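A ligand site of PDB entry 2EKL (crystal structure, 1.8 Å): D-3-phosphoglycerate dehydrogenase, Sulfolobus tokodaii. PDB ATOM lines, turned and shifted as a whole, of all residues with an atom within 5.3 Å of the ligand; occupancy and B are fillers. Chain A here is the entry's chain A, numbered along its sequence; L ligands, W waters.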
ATOM      1  N   ILE A  77      21.780   1.142   9.389  1.00  0.00           N
ATOM      2  CA  ILE A  77      22.128   2.042   8.305  1.00  0.00           C
ATOM      3  C   ILE A  77      20.999   2.994   7.921  1.00  0.00           C
ATOM      4  O   ILE A  77      21.154   3.821   7.033  1.00  0.00           O
ATOM      5  CB  ILE A  77      22.553   1.241   7.057  1.00  0.00           C
ATOM      6  CG1 ILE A  77      21.391   0.377   6.578  1.00  0.00           C
ATOM      7  CG2 ILE A  77      23.757   0.361   7.395  1.00  0.00           C
ATOM      8  CD1 ILE A  77      21.711  -0.473   5.365  1.00  0.00           C
ATOM      9  N   GLY A  99      25.930   5.064   5.551  1.00  0.00           N
ATOM     10  CA  GLY A  99      26.980   4.669   4.618  1.00  0.00           C
ATOM     11  C   GLY A  99      27.834   3.499   5.063  1.00  0.00           C
ATOM     12  O   GLY A  99      28.732   3.082   4.341  1.00  0.00           O
ATOM     13  N   SER A 101      27.451   0.348   5.087  1.00  0.00           N
ATOM     14  CA  SER A 101      27.450  -0.878   4.300  1.00  0.00           C
ATOM     15  C   SER A 101      27.669  -0.683   2.802  1.00  0.00           C
ATOM     16  O   SER A 101      27.520  -1.633   2.026  1.00  0.00           O
ATOM     17  CB  SER A 101      26.123  -1.617   4.511  1.00  0.00           C
ATOM     18  OG  SER A 101      25.052  -0.942   3.873  1.00  0.00           O
ATOM     19  N   THR A 102      28.046   0.525   2.395  1.00  0.00           N
ATOM     20  CA  THR A 102      28.249   0.827   0.982  1.00  0.00           C
ATOM     21  C   THR A 102      28.908  -0.252   0.122  1.00  0.00           C
ATOM     22  O   THR A 102      28.298  -0.759  -0.823  1.00  0.00           O
ATOM     23  CB  THR A 102      29.050   2.139   0.802  1.00  0.00           C
ATOM     24  OG1 THR A 102      28.330   3.218   1.414  1.00  0.00           O
ATOM     25  CG2 THR A 102      29.235   2.447  -0.682  1.00  0.00           C
ATOM     26  N   ALA A 105      26.907  -3.471  -0.262  1.00  0.00           N
ATOM     27  CA  ALA A 105      25.731  -3.313  -1.116  1.00  0.00           C
ATOM     28  C   ALA A 105      26.166  -3.233  -2.573  1.00  0.00           C
ATOM     29  O   ALA A 105      25.503  -3.787  -3.461  1.00  0.00           O
ATOM     30  CB  ALA A 105      24.948  -2.046  -0.716  1.00  0.00           C
ATOM     31  N   VAL A 148      20.587   4.622 -11.851  1.00  0.00           N
ATOM     32  CA  VAL A 148      19.545   5.549 -11.390  1.00  0.00           C
ATOM     33  C   VAL A 148      19.765   5.753  -9.887  1.00  0.00           C
ATOM     34  O   VAL A 148      19.492   4.863  -9.083  1.00  0.00           O
ATOM     35  CB  VAL A 148      18.133   4.982 -11.631  1.00  0.00           C
ATOM     36  CG1 VAL A 148      17.093   6.003 -11.208  1.00  0.00           C
ATOM     37  CG2 VAL A 148      17.969   4.611 -13.089  1.00  0.00           C
ATOM     38  N   GLY A 149      20.254   6.933  -9.524  1.00  0.00           N
ATOM     39  CA  GLY A 149      20.563   7.212  -8.141  1.00  0.00           C
ATOM     40  C   GLY A 149      22.075   7.087  -8.083  1.00  0.00           C
ATOM     41  O   GLY A 149      22.622   5.997  -7.947  1.00  0.00           O
ATOM     42  N   PHE A 150      22.762   8.216  -8.212  1.00  0.00           N
ATOM     43  CA  PHE A 150      24.225   8.234  -8.255  1.00  0.00           C
ATOM     44  C   PHE A 150      24.854   8.705  -6.946  1.00  0.00           C
ATOM     45  O   PHE A 150      25.589   9.693  -6.921  1.00  0.00           O
ATOM     46  CB  PHE A 150      24.669   9.137  -9.416  1.00  0.00           C
ATOM     47  CG  PHE A 150      26.044   8.825  -9.940  1.00  0.00           C
ATOM     48  CD1 PHE A 150      26.308   7.606 -10.551  1.00  0.00           C
ATOM     49  CD2 PHE A 150      27.058   9.771  -9.856  1.00  0.00           C
ATOM     50  CE1 PHE A 150      27.580   7.326 -11.075  1.00  0.00           C
ATOM     51  CE2 PHE A 150      28.330   9.507 -10.373  1.00  0.00           C
ATOM     52  CZ  PHE A 150      28.580   8.287 -10.982  1.00  0.00           C
ATOM     53  N   GLY A 151      24.557   7.992  -5.853  1.00  0.00           N
ATOM     54  CA  GLY A 151      25.104   8.365  -4.564  1.00  0.00           C
ATOM     55  C   GLY A 151      26.291   7.499  -4.184  1.00  0.00           C
ATOM     56  O   GLY A 151      27.072   7.112  -5.038  1.00  0.00           O
ATOM     57  N   ARG A 152      26.415   7.181  -2.888  1.00  0.00           N
ATOM     58  CA  ARG A 152      27.521   6.359  -2.412  1.00  0.00           C
ATOM     59  C   ARG A 152      27.644   5.048  -3.180  1.00  0.00           C
ATOM     60  O   ARG A 152      28.695   4.722  -3.715  1.00  0.00           O
ATOM     61  CB  ARG A 152      27.340   6.022  -0.923  1.00  0.00           C
ATOM     62  CG  ARG A 152      27.173   7.206   0.009  1.00  0.00           C
ATOM     63  CD  ARG A 152      27.325   6.736   1.453  1.00  0.00           C
ATOM     64  NE  ARG A 152      26.990   7.766   2.428  1.00  0.00           N
ATOM     65  CZ  ARG A 152      25.761   8.065   2.830  1.00  0.00           C
ATOM     66  NH1 ARG A 152      24.723   7.411   2.325  1.00  0.00           N
ATOM     67  NH2 ARG A 152      25.564   9.009   3.730  1.00  0.00           N
ATOM     68  N   ILE A 153      26.546   4.297  -3.206  1.00  0.00           N
ATOM     69  CA  ILE A 153      26.520   2.996  -3.872  1.00  0.00           C
ATOM     70  C   ILE A 153      26.490   3.111  -5.390  1.00  0.00           C
ATOM     71  O   ILE A 153      27.253   2.440  -6.085  1.00  0.00           O
ATOM     72  CB  ILE A 153      25.310   2.165  -3.383  1.00  0.00           C
ATOM     73  CG1 ILE A 153      25.476   1.885  -1.895  1.00  0.00           C
ATOM     74  CG2 ILE A 153      25.209   0.852  -4.159  1.00  0.00           C
ATOM     75  CD1 ILE A 153      24.245   1.297  -1.243  1.00  0.00           C
ATOM     76  N   GLY A 154      25.604   3.962  -5.914  1.00  0.00           N
ATOM     77  CA  GLY A 154      25.505   4.121  -7.349  1.00  0.00           C
ATOM     78  C   GLY A 154      26.823   4.485  -8.012  1.00  0.00           C
ATOM     79  O   GLY A 154      27.164   3.960  -9.074  1.00  0.00           O
ATOM     80  N   TYR A 171      21.772   8.906 -13.831  1.00  0.00           N
ATOM     81  CA  TYR A 171      20.734   9.912 -13.621  1.00  0.00           C
ATOM     82  C   TYR A 171      20.510  10.070 -12.127  1.00  0.00           C
ATOM     83  O   TYR A 171      20.457   9.098 -11.381  1.00  0.00           O
ATOM     84  CB  TYR A 171      19.403   9.514 -14.266  1.00  0.00           C
ATOM     85  CG  TYR A 171      18.281  10.454 -13.846  1.00  0.00           C
ATOM     86  CD1 TYR A 171      18.268  11.787 -14.260  1.00  0.00           C
ATOM     87  CD2 TYR A 171      17.259  10.024 -12.988  1.00  0.00           C
ATOM     88  CE1 TYR A 171      17.284  12.675 -13.810  1.00  0.00           C
ATOM     89  CE2 TYR A 171      16.267  10.902 -12.545  1.00  0.00           C
ATOM     90  CZ  TYR A 171      16.283  12.223 -12.961  1.00  0.00           C
ATOM     91  OH  TYR A 171      15.332  13.103 -12.494  1.00  0.00           O
ATOM     92  N   ASP A 172      20.385  11.327 -11.709  1.00  0.00           N
ATOM     93  CA  ASP A 172      20.126  11.629 -10.319  1.00  0.00           C
ATOM     94  C   ASP A 172      19.362  12.943 -10.321  1.00  0.00           C
ATOM     95  O   ASP A 172      19.522  13.745 -11.236  1.00  0.00           O
ATOM     96  CB  ASP A 172      21.433  11.767  -9.540  1.00  0.00           C
ATOM     97  CG  ASP A 172      21.238  11.647  -8.039  1.00  0.00           C
ATOM     98  OD1 ASP A 172      20.551  12.516  -7.454  1.00  0.00           O
ATOM     99  OD2 ASP A 172      21.763  10.678  -7.450  1.00  0.00           O
ATOM    100  N   ILE A 173      18.500  13.143  -9.337  1.00  0.00           N
ATOM    101  CA  ILE A 173      17.737  14.382  -9.274  1.00  0.00           C
ATOM    102  C   ILE A 173      18.673  15.519  -8.876  1.00  0.00           C
ATOM    103  O   ILE A 173      18.402  16.687  -9.138  1.00  0.00           O
ATOM    104  CB  ILE A 173      16.583  14.279  -8.283  1.00  0.00           C
ATOM    105  CG1 ILE A 173      17.100  13.871  -6.904  1.00  0.00           C
ATOM    106  CG2 ILE A 173      15.554  13.277  -8.796  1.00  0.00           C
ATOM    107  CD1 ILE A 173      16.028  13.742  -5.859  1.00  0.00           C
ATOM    108  N   LEU A 174      19.785  15.142  -8.248  1.00  0.00           N
ATOM    109  CA  LEU A 174      20.781  16.119  -7.818  1.00  0.00           C
ATOM    110  C   LEU A 174      21.820  16.285  -8.917  1.00  0.00           C
ATOM    111  O   LEU A 174      21.930  15.455  -9.815  1.00  0.00           O
ATOM    112  CB  LEU A 174      21.467  15.647  -6.534  1.00  0.00           C
ATOM    113  CG  LEU A 174      20.604  15.458  -5.292  1.00  0.00           C
ATOM    114  CD1 LEU A 174      21.471  14.997  -4.129  1.00  0.00           C
ATOM    115  CD2 LEU A 174      19.889  16.758  -4.949  1.00  0.00           C
ATOM    116  N   HIS A 203      19.595   2.689  -7.290  1.00  0.00           N
ATOM    117  CA  HIS A 203      20.299   2.985  -6.040  1.00  0.00           C
ATOM    118  C   HIS A 203      19.800   4.297  -5.464  1.00  0.00           C
ATOM    119  O   HIS A 203      20.587   5.134  -5.007  1.00  0.00           O
ATOM    120  CB  HIS A 203      21.798   3.074  -6.318  1.00  0.00           C
ATOM    121  CG  HIS A 203      22.354   1.845  -6.950  1.00  0.00           C
ATOM    122  ND1 HIS A 203      22.553   0.675  -6.244  1.00  0.00           N
ATOM    123  CD2 HIS A 203      22.692   1.576  -8.234  1.00  0.00           C
ATOM    124  CE1 HIS A 203      22.978  -0.262  -7.066  1.00  0.00           C
ATOM    125  NE2 HIS A 203      23.075   0.259  -8.278  1.00  0.00           N
ATOM    126  N   VAL A 204      18.486   4.473  -5.469  1.00  0.00           N
ATOM    127  CA  VAL A 204      17.864   5.699  -4.981  1.00  0.00           C
ATOM    128  C   VAL A 204      17.374   5.647  -3.542  1.00  0.00           C
ATOM    129  O   VAL A 204      17.155   4.568  -2.988  1.00  0.00           O
ATOM    130  CB  VAL A 204      16.648   6.088  -5.853  1.00  0.00           C
ATOM    131  CG1 VAL A 204      17.090   6.301  -7.294  1.00  0.00           C
ATOM    132  CG2 VAL A 204      15.585   4.993  -5.768  1.00  0.00           C
ATOM    133  N   THR A 205      17.217   6.822  -2.959  1.00  0.00           N
ATOM    134  CA  THR A 205      16.683   6.966  -1.613  1.00  0.00           C
ATOM    135  C   THR A 205      15.318   7.607  -1.821  1.00  0.00           C
ATOM    136  O   THR A 205      15.218   8.743  -2.278  1.00  0.00           O
ATOM    137  CB  THR A 205      17.536   7.917  -0.745  1.00  0.00           C
ATOM    138  OG1 THR A 205      17.740   9.148  -1.460  1.00  0.00           O
ATOM    139  CG2 THR A 205      18.866   7.282  -0.399  1.00  0.00           C
ATOM    140  N   VAL A 206      14.266   6.854  -1.514  1.00  0.00           N
ATOM    141  CA  VAL A 206      12.912   7.338  -1.674  1.00  0.00           C
ATOM    142  C   VAL A 206      12.086   6.991  -0.448  1.00  0.00           C
ATOM    143  O   VAL A 206      12.447   6.093   0.316  1.00  0.00           O
ATOM    144  CB  VAL A 206      12.240   6.722  -2.919  1.00  0.00           C
ATOM    145  CG1 VAL A 206      12.944   7.187  -4.179  1.00  0.00           C
ATOM    146  CG2 VAL A 206      12.286   5.205  -2.835  1.00  0.00           C
ATOM    147  N   ILE A 213       9.561   5.483  -9.026  1.00  0.00           N
ATOM    148  CA  ILE A 213      10.330   6.216 -10.028  1.00  0.00           C
ATOM    149  C   ILE A 213      10.281   5.456 -11.347  1.00  0.00           C
ATOM    150  O   ILE A 213      10.303   6.044 -12.418  1.00  0.00           O
ATOM    151  CB  ILE A 213      11.789   6.390  -9.586  1.00  0.00           C
ATOM    152  CG1 ILE A 213      11.833   7.177  -8.281  1.00  0.00           C
ATOM    153  CG2 ILE A 213      12.580   7.118 -10.673  1.00  0.00           C
ATOM    154  CD1 ILE A 213      11.097   8.493  -8.329  1.00  0.00           C
ATOM    155  N   THR A 231      18.886  -2.914  -5.542  1.00  0.00           N
ATOM    156  CA  THR A 231      19.362  -3.201  -4.191  1.00  0.00           C
ATOM    157  C   THR A 231      19.071  -1.994  -3.306  1.00  0.00           C
ATOM    158  O   THR A 231      19.607  -1.885  -2.202  1.00  0.00           O
ATOM    159  CB  THR A 231      20.884  -3.486  -4.145  1.00  0.00           C
ATOM    160  OG1 THR A 231      21.603  -2.385  -4.705  1.00  0.00           O
ATOM    161  CG2 THR A 231      21.206  -4.761  -4.908  1.00  0.00           C
ATOM    162  N   SER A 232      18.225  -1.096  -3.783  1.00  0.00           N
ATOM    163  CA  SER A 232      17.872   0.098  -3.021  1.00  0.00           C
ATOM    164  C   SER A 232      16.557  -0.076  -2.260  1.00  0.00           C
ATOM    165  O   SER A 232      16.573  -0.492  -1.094  1.00  0.00           O
ATOM    166  CB  SER A 232      17.814   1.324  -3.943  1.00  0.00           C
ATOM    167  OG  SER A 232      16.848   1.169  -4.975  1.00  0.00           O
ATOM    168  N   ARG A 233      15.439   0.248  -2.897  1.00  0.00           N
ATOM    169  CA  ARG A 233      14.129   0.109  -2.267  1.00  0.00           C
ATOM    170  C   ARG A 233      13.108  -0.468  -3.253  1.00  0.00           C
ATOM    171  O   ARG A 233      13.065  -0.068  -4.412  1.00  0.00           O
ATOM    172  CB  ARG A 233      13.604   1.451  -1.754  1.00  0.00           C
ATOM    173  CG  ARG A 233      14.238   1.914  -0.454  1.00  0.00           C
ATOM    174  CD  ARG A 233      13.286   2.828   0.294  1.00  0.00           C
ATOM    175  NE  ARG A 233      13.808   3.250   1.588  1.00  0.00           N
ATOM    176  CZ  ARG A 233      13.123   3.954   2.471  1.00  0.00           C
ATOM    177  NH1 ARG A 233      11.870   4.308   2.208  1.00  0.00           N
ATOM    178  NH2 ARG A 233      13.678   4.305   3.629  1.00  0.00           N
ATOM    179  N   ASP A 257      17.410  -7.368  -4.207  1.00  0.00           N
ATOM    180  CA  ASP A 257      17.737  -7.769  -2.843  1.00  0.00           C
ATOM    181  C   ASP A 257      16.586  -7.262  -1.957  1.00  0.00           C
ATOM    182  O   ASP A 257      16.568  -7.517  -0.755  1.00  0.00           O
ATOM    183  CB  ASP A 257      19.056  -7.139  -2.395  1.00  0.00           C
ATOM    184  CG  ASP A 257      19.469  -7.577  -1.006  1.00  0.00           C
ATOM    185  OD1 ASP A 257      19.495  -8.804  -0.737  1.00  0.00           O
ATOM    186  OD2 ASP A 257      19.784  -6.707  -0.167  1.00  0.00           O
ATOM    187  N   VAL A 258      15.654  -6.546  -2.562  1.00  0.00           N
ATOM    188  CA  VAL A 258      14.523  -5.985  -1.834  1.00  0.00           C
ATOM    189  C   VAL A 258      13.165  -6.307  -2.478  1.00  0.00           C
ATOM    190  O   VAL A 258      13.000  -6.225  -3.693  1.00  0.00           O
ATOM    191  CB  VAL A 258      14.662  -4.448  -1.702  1.00  0.00           C
ATOM    192  CG1 VAL A 258      15.915  -4.110  -0.901  1.00  0.00           C
ATOM    193  CG2 VAL A 258      14.716  -3.810  -3.084  1.00  0.00           C
ATOM    194  N   HIS A 283      17.427  -9.642   1.206  1.00  0.00           N
ATOM    195  CA  HIS A 283      17.828  -8.377   1.823  1.00  0.00           C
ATOM    196  C   HIS A 283      19.129  -8.527   2.606  1.00  0.00           C
ATOM    197  O   HIS A 283      19.218  -8.156   3.778  1.00  0.00           O
ATOM    198  CB  HIS A 283      16.703  -7.870   2.736  1.00  0.00           C
ATOM    199  CG  HIS A 283      16.622  -6.377   2.826  1.00  0.00           C
ATOM    200  ND1 HIS A 283      15.427  -5.701   2.802  1.00  0.00           N
ATOM    201  CD2 HIS A 283      17.585  -5.445   2.941  1.00  0.00           C
ATOM    202  CE1 HIS A 283      15.668  -4.401   2.881  1.00  0.00           C
ATOM    203  NE2 HIS A 283      16.969  -4.217   2.974  1.00  0.00           N
ATOM    204  N   ILE A 284      20.136  -9.077   1.925  1.00  0.00           N
ATOM    205  CA  ILE A 284      21.441  -9.302   2.526  1.00  0.00           C
ATOM    206  C   ILE A 284      22.491  -8.274   2.106  1.00  0.00           C
ATOM    207  O   ILE A 284      23.677  -8.474   2.339  1.00  0.00           O
ATOM    208  CB  ILE A 284      21.965 -10.707   2.148  1.00  0.00           C
ATOM    209  CG1 ILE A 284      22.053 -10.855   0.621  1.00  0.00           C
ATOM    210  CG2 ILE A 284      21.031 -11.783   2.725  1.00  0.00           C
ATOM    211  CD1 ILE A 284      22.636 -12.175   0.157  1.00  0.00           C
ATOM    212  N   GLY A 285      22.047  -7.176   1.501  1.00  0.00           N
ATOM    213  CA  GLY A 285      22.969  -6.145   1.048  1.00  0.00           C
ATOM    214  C   GLY A 285      23.964  -5.628   2.069  1.00  0.00           C
ATOM    215  O   GLY A 285      25.111  -5.307   1.716  1.00  0.00           O
ATOM    216  N   ALA A 286      23.564  -5.529   3.332  1.00  0.00           N
ATOM    217  CA  ALA A 286      24.445  -5.054   4.388  1.00  0.00           C
ATOM    218  C   ALA A 286      24.900  -6.212   5.260  1.00  0.00           C
ATOM    219  O   ALA A 286      25.553  -6.011   6.287  1.00  0.00           O
ATOM    220  CB  ALA A 286      23.717  -4.012   5.245  1.00  0.00           C
HETATM  221  P1  LIG L   1      22.792   8.003  -1.153  1.00  0.00           P
HETATM  222  O1  LIG L   1      24.269   8.147  -1.099  1.00  0.00           O
HETATM  223  O2  LIG L   1      21.994   8.977  -0.315  1.00  0.00           O
HETATM  224  O3  LIG L   1      22.387   8.091  -2.694  1.00  0.00           O
HETATM  225  C1  LIG L   1      21.005   8.025  -3.054  1.00  0.00           C
HETATM  226  C2  LIG L   1      20.932   8.885  -4.460  1.00  0.00           C
HETATM  227  O4  LIG L   1      19.712   8.603  -5.163  1.00  0.00           O
HETATM  228  C3  LIG L   1      21.138  10.411  -4.182  1.00  0.00           C
HETATM  229  O5  LIG L   1      22.174  10.952  -4.991  1.00  0.00           O
HETATM  230  C4  LIG L   1      19.724  10.962  -4.417  1.00  0.00           C
HETATM  231  O6  LIG L   1      19.603  12.324  -4.770  1.00  0.00           O
HETATM  232  C5  LIG L   1      19.262   9.977  -5.418  1.00  0.00           C
HETATM  233  N1  LIG L   1      17.785  10.002  -5.658  1.00  0.00           N
HETATM  234  C6  LIG L   1      16.719  10.127  -4.774  1.00  0.00           C
HETATM  235  N2  LIG L   1      15.561  10.107  -5.464  1.00  0.00           N
HETATM  236  C7  LIG L   1      15.848   9.979  -6.778  1.00  0.00           C
HETATM  237  C8  LIG L   1      15.082   9.891  -8.006  1.00  0.00           C
HETATM  238  N3  LIG L   1      13.760   9.948  -7.987  1.00  0.00           N
HETATM  239  N4  LIG L   1      15.751   9.753  -9.271  1.00  0.00           N
HETATM  240  C9  LIG L   1      17.177   9.695  -9.356  1.00  0.00           C
HETATM  241  N5  LIG L   1      17.931   9.769  -8.165  1.00  0.00           N
HETATM  242  C10 LIG L   1      17.275   9.906  -6.912  1.00  0.00           C
HETATM  243  O7  LIG L   1      22.385   6.527  -0.651  1.00  0.00           O
HETATM  244  P2  LIG L   1      23.172   5.129  -0.770  1.00  0.00           P
HETATM  245  O8  LIG L   1      23.958   5.101  -2.011  1.00  0.00           O
HETATM  246  O9  LIG L   1      23.964   5.033   0.499  1.00  0.00           O
HETATM  247  O10 LIG L   1      21.923   4.169  -0.713  1.00  0.00           O
HETATM  248  C11 LIG L   1      21.160   3.959  -1.888  1.00  0.00           C
HETATM  249  C12 LIG L   1      19.992   3.036  -1.625  1.00  0.00           C
HETATM  250  O11 LIG L   1      20.422   1.731  -1.246  1.00  0.00           O
HETATM  251  C13 LIG L   1      19.008   3.465  -0.492  1.00  0.00           C
HETATM  252  O12 LIG L   1      17.640   3.244  -0.886  1.00  0.00           O
HETATM  253  C14 LIG L   1      19.456   2.660   0.674  1.00  0.00           C
HETATM  254  O13 LIG L   1      18.505   2.660   1.729  1.00  0.00           O
HETATM  255  C15 LIG L   1      19.735   1.379  -0.051  1.00  0.00           C
HETATM  256  N6  LIG L   1      20.580   0.358   0.635  1.00  0.00           N
HETATM  257  C16 LIG L   1      20.141  -1.008   0.587  1.00  0.00           C
HETATM  258  C17 LIG L   1      20.937  -1.996   1.242  1.00  0.00           C
HETATM  259  C18 LIG L   1      20.502  -3.419   1.194  1.00  0.00           C
HETATM  260  O14 LIG L   1      20.753  -4.163   2.285  1.00  0.00           O
HETATM  261  N7  LIG L   1      19.875  -3.978   0.168  1.00  0.00           N
HETATM  262  C19 LIG L   1      22.179  -1.563   1.934  1.00  0.00           C
HETATM  263  C20 LIG L   1      22.608  -0.179   1.970  1.00  0.00           C
HETATM  264  C21 LIG L   1      21.791   0.784   1.302  1.00  0.00           C
HETATM  265  O   HOH W   1      20.004  -3.577   4.680  1.00  0.00           O
HETATM  266  O   HOH W   2      22.204   4.268   2.599  1.00  0.00           O
HETATM  267  O   HOH W   3      18.062  13.698  -3.147  1.00  0.00           O
HETATM  268  O   HOH W   4      19.100   2.907   4.422  1.00  0.00           O
HETATM  269  O   HOH W   5      23.483   5.542  -4.677  1.00  0.00           O
HETATM  270  O   HOH W   6      21.124  -6.367   4.661  1.00  0.00           O
HETATM  271  O   HOH W   7      25.620  10.483  -1.728  1.00  0.00           O
HETATM  272  O   HOH W   8      25.534   3.123   1.709  1.00  0.00           O
HETATM  273  O   HOH W   9      13.598  10.955  -3.218  1.00  0.00           O
HETATM  274  O   HOH W  10      16.423  11.711  -1.966  1.00  0.00           O
HETATM  275  O   HOH W  11      19.726  10.642  -0.532  1.00  0.00           O
HETATM  276  O   HOH W  12      23.140  11.247   0.836  1.00  0.00           O
HETATM  277  O   HOH W  13      24.022  12.151  -3.361  1.00  0.00           O
HETATM  278  O   HOH W  14      21.575   0.306  -3.522  1.00  0.00           O
HETATM  279  O   HOH W  15      15.807   4.785   0.789  1.00  0.00           O
HETATM  280  O   HOH W  16      12.545  10.800  -5.820  1.00  0.00           O
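O of Thr 205 lies close to N2 of the ligand (3.5 Å). Ile 77 touches the ligand (CD1 to C20, 3.5 Å). Ser 101 touches the ligand (OG to C20, 3.2 Å). CB of Ala 105 touches C19 of the ligand, 3.9 Å away. Gly 149 touches the ligand. CA of Gly 151 touches O3 of the ligand, 3.3 Å away. Tyr 171 touches the ligand (CE2 to N4, 3.5 Å). Ile 173 touches the ligand (CG2 to C8, 3.5 Å). CD1 of Leu 174 touches O6 of the ligand, at 3.3 Å. His 203 touches the ligand (O to C11, 3.4 Å). CD1 of Ile 213 touches N3 of the ligand, at 3.1 Å. Ser 232 touches the ligand (CA to O11, 3.5 Å). Arg 233 touches the ligand. His 283 touches the ligand (CD2 to O14, 3.5 Å). Hydrophobic or aromatic side chains within 4 Å of the ligand: Ile 77, Ala 105, Ile 153, Tyr 171, Ile 173, Leu 174, Val 204, Ile 213 and His 283. Of the 30 residues printed, 22 come within 4 Å of the ligand. The nearest printed residue that does not touch the ligand is Phe 150 (4.01 Å).
Water W8 lies within hydrogen-bond range of O9 of the ligand (2.8 Å) and OG1 of Thr 102 (2.8 Å). Water W4 lies within hydrogen-bond range of O13 of the ligand and O of Ile 77. Water W15 lies within hydrogen-bond range of the guanidinium group of Arg 233, an oxygen (O12) of the ligand and the backbone NH of Val 206. Water W14 lies within hydrogen-bond range of a ring nitrogen (ND1) of His 203 (2.9 Å), an oxygen (O11) of the ligand (2.9 Å) and the side-chain hydroxyl (OG1) of Thr 231 (2.9 Å). Water W9 lies within hydrogen-bond range of O of Thr 205 (2.9 Å) and N2 of the ligand (3.1 Å). Water W6 lies within hydrogen-bond range of O of His 283 (2.8 Å), N of Ala 286 (2.9 Å), O14 of the ligand (3.3 Å) and N of Gly 285 (3.4 Å).
The side-chain carboxylate (OD2) of Asp 172 sits at hydrogen-bond distance from an oxygen (O5) of the ligand, 2.5 Å away. An oxygen (O12) of the ligand sits at hydrogen-bond distance from the backbone carbonyl oxygen (O) of Val 204, at 2.5 Å. The side-chain carboxylate of Asp 257 lies within hydrogen-bond range of a nitrogen (N7) of the ligand, at 2.8 Å. The backbone NH of Arg 152 sits at hydrogen-bond distance from an oxygen (O1) of the ligand (3.0 Å). NH1 of Arg 152 lies within salt-bridge range of O9 of the ligand (3.1 Å). O8 of the ligand lies within hydrogen-bond range of N of Ile 153, 3.0 Å away. The backbone carbonyl oxygen (O) of Thr 231 sits close to a nitrogen (N7) of the ligand, at 3.2 Å. The backbone NH (N) of Gly 285 lies close to an oxygen (O14) of the ligand, 3.4 Å away. N of Ala 286 is in hydrogen-bond range of O14 of the ligand, 3.3 Å away.
N of Leu 174 sits at hydrogen-bond distance from OD1 of Asp 172 (2.8 Å). The backbone NH (N) of Phe 150 is in hydrogen-bond range of the side-chain carboxylate (OD2) of Asp 172. The side-chain carboxylate of Asp 257 sits at hydrogen-bond distance from the backbone NH of Gly 285. The side-chain carboxylate (OD1) of Asp 257 sits at hydrogen-bond distance from the backbone NH (N) of His 283 (3.0 Å). N of Ile 284 sits at hydrogen-bond distance from OD1 of Asp 257 (2.8 Å). N of Ala 105 sits at hydrogen-bond distance from O of Gly 285, 3.2 Å away. N of His 203 sits at hydrogen-bond distance from O of Val 148, at 2.8 Å. The guanidinium group (NH1) of Arg 233 sits at hydrogen-bond distance from the backbone carbonyl oxygen (O) of Val 206, at 2.7 Å.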
